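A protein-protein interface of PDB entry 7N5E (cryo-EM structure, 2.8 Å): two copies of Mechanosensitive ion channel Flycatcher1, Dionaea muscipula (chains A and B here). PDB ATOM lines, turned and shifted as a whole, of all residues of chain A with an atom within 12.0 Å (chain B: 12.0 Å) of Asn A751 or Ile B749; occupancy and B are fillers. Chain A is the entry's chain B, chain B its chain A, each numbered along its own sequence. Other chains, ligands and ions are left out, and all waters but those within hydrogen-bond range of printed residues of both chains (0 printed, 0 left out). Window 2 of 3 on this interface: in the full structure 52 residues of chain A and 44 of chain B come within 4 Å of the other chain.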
ATOM      1  N   ILE A 747     -25.063  -8.478  -9.850  1.00  0.00           N
ATOM      2  CA  ILE A 747     -24.088  -8.903 -10.824  1.00  0.00           C
ATOM      3  C   ILE A 747     -23.565  -7.796 -11.703  1.00  0.00           C
ATOM      4  O   ILE A 747     -24.297  -6.915 -12.171  1.00  0.00           O
ATOM      5  CB  ILE A 747     -24.685 -10.011 -11.700  1.00  0.00           C
ATOM      6  CG1 ILE A 747     -25.100 -11.215 -10.846  1.00  0.00           C
ATOM      7  CG2 ILE A 747     -23.775 -10.397 -12.812  1.00  0.00           C
ATOM      8  CD1 ILE A 747     -24.021 -11.924 -10.103  1.00  0.00           C
ATOM      9  N   SER A 748     -22.278  -7.820 -11.902  1.00  0.00           N
ATOM     10  CA  SER A 748     -21.676  -6.859 -12.779  1.00  0.00           C
ATOM     11  C   SER A 748     -20.905  -7.599 -13.819  1.00  0.00           C
ATOM     12  O   SER A 748     -19.914  -8.251 -13.513  1.00  0.00           O
ATOM     13  CB  SER A 748     -20.778  -5.950 -12.013  1.00  0.00           C
ATOM     14  OG  SER A 748     -20.160  -5.051 -12.866  1.00  0.00           O
ATOM     15  N   ILE A 749     -21.342  -7.532 -15.059  1.00  0.00           N
ATOM     16  CA  ILE A 749     -20.660  -8.296 -16.062  1.00  0.00           C
ATOM     17  C   ILE A 749     -19.603  -7.462 -16.721  1.00  0.00           C
ATOM     18  O   ILE A 749     -19.872  -6.440 -17.342  1.00  0.00           O
ATOM     19  CB  ILE A 749     -21.632  -8.822 -17.120  1.00  0.00           C
ATOM     20  CG1 ILE A 749     -22.664  -9.690 -16.431  1.00  0.00           C
ATOM     21  CG2 ILE A 749     -20.869  -9.617 -18.166  1.00  0.00           C
ATOM     22  CD1 ILE A 749     -23.835 -10.069 -17.265  1.00  0.00           C
ATOM     23  N   ARG A 750     -18.392  -7.941 -16.575  1.00  0.00           N
ATOM     24  CA  ARG A 750     -17.185  -7.352 -17.127  1.00  0.00           C
ATOM     25  C   ARG A 750     -17.079  -7.540 -18.651  1.00  0.00           C
ATOM     26  O   ARG A 750     -16.523  -6.684 -19.338  1.00  0.00           O
ATOM     27  CB  ARG A 750     -15.975  -7.968 -16.441  1.00  0.00           C
ATOM     28  CG  ARG A 750     -14.591  -7.515 -16.906  1.00  0.00           C
ATOM     29  CD  ARG A 750     -14.312  -6.075 -16.642  1.00  0.00           C
ATOM     30  NE  ARG A 750     -14.264  -5.774 -15.204  1.00  0.00           N
ATOM     31  CZ  ARG A 750     -14.185  -4.534 -14.666  1.00  0.00           C
ATOM     32  NH1 ARG A 750     -14.132  -3.464 -15.445  1.00  0.00           N
ATOM     33  NH2 ARG A 750     -14.162  -4.394 -13.347  1.00  0.00           N
ATOM     34  N   ASN A 751     -17.581  -8.700 -19.161  1.00  0.00           N
ATOM     35  CA  ASN A 751     -17.604  -9.189 -20.543  1.00  0.00           C
ATOM     36  C   ASN A 751     -16.260  -9.816 -20.853  1.00  0.00           C
ATOM     37  O   ASN A 751     -16.013 -10.970 -20.488  1.00  0.00           O
ATOM     38  CB  ASN A 751     -18.004  -8.100 -21.589  1.00  0.00           C
ATOM     39  CG  ASN A 751     -19.508  -7.572 -21.428  1.00  0.00           C
ATOM     40  OD1 ASN A 751     -20.443  -8.391 -21.315  1.00  0.00           O
ATOM     41  ND2 ASN A 751     -19.709  -6.228 -21.418  1.00  0.00           N
ATOM     42  N   GLN B 745     -21.037  -9.453  -7.240  1.00  0.00           N
ATOM     43  CA  GLN B 745     -20.149 -10.404  -7.872  1.00  0.00           C
ATOM     44  C   GLN B 745     -19.852 -10.044  -9.300  1.00  0.00           C
ATOM     45  O   GLN B 745     -20.765  -9.931 -10.120  1.00  0.00           O
ATOM     46  CB  GLN B 745     -20.761 -11.791  -7.793  1.00  0.00           C
ATOM     47  CG  GLN B 745     -20.006 -12.868  -8.479  1.00  0.00           C
ATOM     48  CD  GLN B 745     -18.748 -13.216  -7.808  1.00  0.00           C
ATOM     49  OE1 GLN B 745     -18.749 -13.662  -6.666  1.00  0.00           O
ATOM     50  NE2 GLN B 745     -17.654 -13.021  -8.499  1.00  0.00           N
ATOM     51  N   GLU B 746     -18.579  -9.878  -9.601  1.00  0.00           N
ATOM     52  CA  GLU B 746     -18.162  -9.585 -10.955  1.00  0.00           C
ATOM     53  C   GLU B 746     -18.076 -10.858 -11.754  1.00  0.00           C
ATOM     54  O   GLU B 746     -17.534 -11.853 -11.266  1.00  0.00           O
ATOM     55  CB  GLU B 746     -16.840  -8.868 -10.997  1.00  0.00           C
ATOM     56  CG  GLU B 746     -16.416  -8.561 -12.383  1.00  0.00           C
ATOM     57  CD  GLU B 746     -15.218  -7.751 -12.464  1.00  0.00           C
ATOM     58  OE1 GLU B 746     -15.136  -6.768 -11.782  1.00  0.00           O
ATOM     59  OE2 GLU B 746     -14.344  -8.093 -13.216  1.00  0.00           O
ATOM     60  N   ILE B 747     -18.635 -10.821 -12.951  1.00  0.00           N
ATOM     61  CA  ILE B 747     -18.692 -11.939 -13.867  1.00  0.00           C
ATOM     62  C   ILE B 747     -17.995 -11.680 -15.180  1.00  0.00           C
ATOM     63  O   ILE B 747     -18.146 -10.628 -15.790  1.00  0.00           O
ATOM     64  CB  ILE B 747     -20.146 -12.313 -14.140  1.00  0.00           C
ATOM     65  CG1 ILE B 747     -20.869 -12.668 -12.869  1.00  0.00           C
ATOM     66  CG2 ILE B 747     -20.251 -13.371 -15.138  1.00  0.00           C
ATOM     67  CD1 ILE B 747     -20.380 -13.835 -12.109  1.00  0.00           C
ATOM     68  N   SER B 748     -17.220 -12.643 -15.612  1.00  0.00           N
ATOM     69  CA  SER B 748     -16.527 -12.590 -16.892  1.00  0.00           C
ATOM     70  C   SER B 748     -17.119 -13.666 -17.770  1.00  0.00           C
ATOM     71  O   SER B 748     -17.383 -14.758 -17.278  1.00  0.00           O
ATOM     72  CB  SER B 748     -15.059 -12.811 -16.689  1.00  0.00           C
ATOM     73  OG  SER B 748     -14.403 -12.892 -17.903  1.00  0.00           O
ATOM     74  N   ILE B 749     -17.438 -13.370 -19.028  1.00  0.00           N
ATOM     75  CA  ILE B 749     -18.061 -14.407 -19.851  1.00  0.00           C
ATOM     76  C   ILE B 749     -17.177 -14.852 -20.983  1.00  0.00           C
ATOM     77  O   ILE B 749     -16.794 -14.062 -21.845  1.00  0.00           O
ATOM     78  CB  ILE B 749     -19.394 -13.947 -20.476  1.00  0.00           C
ATOM     79  CG1 ILE B 749     -20.390 -13.456 -19.421  1.00  0.00           C
ATOM     80  CG2 ILE B 749     -20.002 -15.091 -21.306  1.00  0.00           C
ATOM     81  CD1 ILE B 749     -20.819 -14.462 -18.393  1.00  0.00           C
ATOM     82  N   ARG B 750     -16.917 -16.138 -21.037  1.00  0.00           N
ATOM     83  CA  ARG B 750     -16.116 -16.676 -22.104  1.00  0.00           C
ATOM     84  C   ARG B 750     -17.051 -17.371 -23.090  1.00  0.00           C
ATOM     85  O   ARG B 750     -17.559 -18.457 -22.801  1.00  0.00           O
ATOM     86  CB  ARG B 750     -15.081 -17.639 -21.571  1.00  0.00           C
ATOM     87  CG  ARG B 750     -14.127 -18.156 -22.620  1.00  0.00           C
ATOM     88  CD  ARG B 750     -13.100 -19.045 -22.045  1.00  0.00           C
ATOM     89  NE  ARG B 750     -12.258 -18.340 -21.093  1.00  0.00           N
ATOM     90  CZ  ARG B 750     -11.184 -17.564 -21.383  1.00  0.00           C
ATOM     91  NH1 ARG B 750     -10.788 -17.378 -22.635  1.00  0.00           N
ATOM     92  NH2 ARG B 750     -10.530 -16.985 -20.383  1.00  0.00           N
ATOM     93  N   ASN B 751     -17.289 -16.735 -24.262  1.00  0.00           N
ATOM     94  CA  ASN B 751     -18.210 -17.168 -25.329  1.00  0.00           C
ATOM     95  C   ASN B 751     -19.630 -17.403 -24.784  1.00  0.00           C
ATOM     96  O   ASN B 751     -20.555 -16.634 -25.071  1.00  0.00           O
ATOM     97  CB  ASN B 751     -17.677 -18.427 -26.080  1.00  0.00           C
ATOM     98  CG  ASN B 751     -16.341 -18.180 -26.927  1.00  0.00           C
ATOM     99  OD1 ASN B 751     -16.082 -17.052 -27.394  1.00  0.00           O
ATOM    100  ND2 ASN B 751     -15.521 -19.244 -27.113  1.00  0.00           N
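Among the printed residues, pairs that only touch across the chains: Ser A748 with Glu B746, Ile A749 with Ile B747, Ile A747 with Gln B745, Asn A751 with Ser B748, Ile A747 with Ile B747 and Asn A751 with Ile B747.
Of the 7 printed residues of chain B, 5 touch a printed residue of chain A. Hydrophobic or aromatic side chains of chain B within 4 Å of the printed part of chain A: Ile B747. Among the printed residues, 11 pairs touch across the chains. Among the printed residues, Asp or Glu carboxylates within 4 Å of a Lys or Arg side-chain nitrogen of the other chain: Arg A750 with Glu B746 (3.0 Å).
Ile A747 touches its own counterpart, Ile B747. Ser A748 touches Ile B747, but with the chains exchanged Ile A747 does not touch Ser B748 (7.5 Å). Asn A751 touches Ser B748, but with the chains exchanged Ser A748 does not touch Asn B751 (13.9 Å). Asn A751 touches Ile B749, but with the chains exchanged Ile A749 does not touch Asn B751 (9.8 Å). Positions printed for both chains: 747, 748, 749, 750 and 751.
Of the printed residues of chain B, Ile A747 touches Gln B745 (3.5 Å) and Ile B747 (3.7 Å). Of the printed residues of chain B, Arg A750 touches Glu B746 (3.0 Å) and Ile B747 (2.8 Å). Asn A751 touches just these residues of chain B: Ile B747, Ser B748 and Ile B749. Ile B747 touches just these residues of chain A: Ile A747, Ser A748, Ile A749, Arg A750 and Asn A751. Of chain A, only Asn A751 (3.1 Å) comes within 4 Å of Ile B749. No residue of chain A comes within 4 Å of Arg B750. No residue of chain A comes within 4 Å of Asn B751. The nearest residue of chain B that does not touch Asn A751 is Arg B750 (5.3 Å). The nearest residue of chain A that does not touch Ile B749 is Ile A749 (4.1 Å).
The backbone NH of Ile B747 lies within hydrogen-bond range of the backbone carbonyl oxygen of Ser A748. The backbone NH (N) of Arg A750 sits at hydrogen-bond distance from the backbone carbonyl oxygen (O) of Ile B747 (2.8 Å). The backbone carbonyl oxygen (O) of Asn A751 lies within hydrogen-bond range of the backbone NH (N) of Ile B749. NH2 of Arg A750 is in salt-bridge range of OE1 of Glu B746, at 3.0 Å. The backbone NH (N) of Ser A748 lies within hydrogen-bond range of the backbone carbonyl oxygen (O) of Gln B745, 3.1 Å away.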
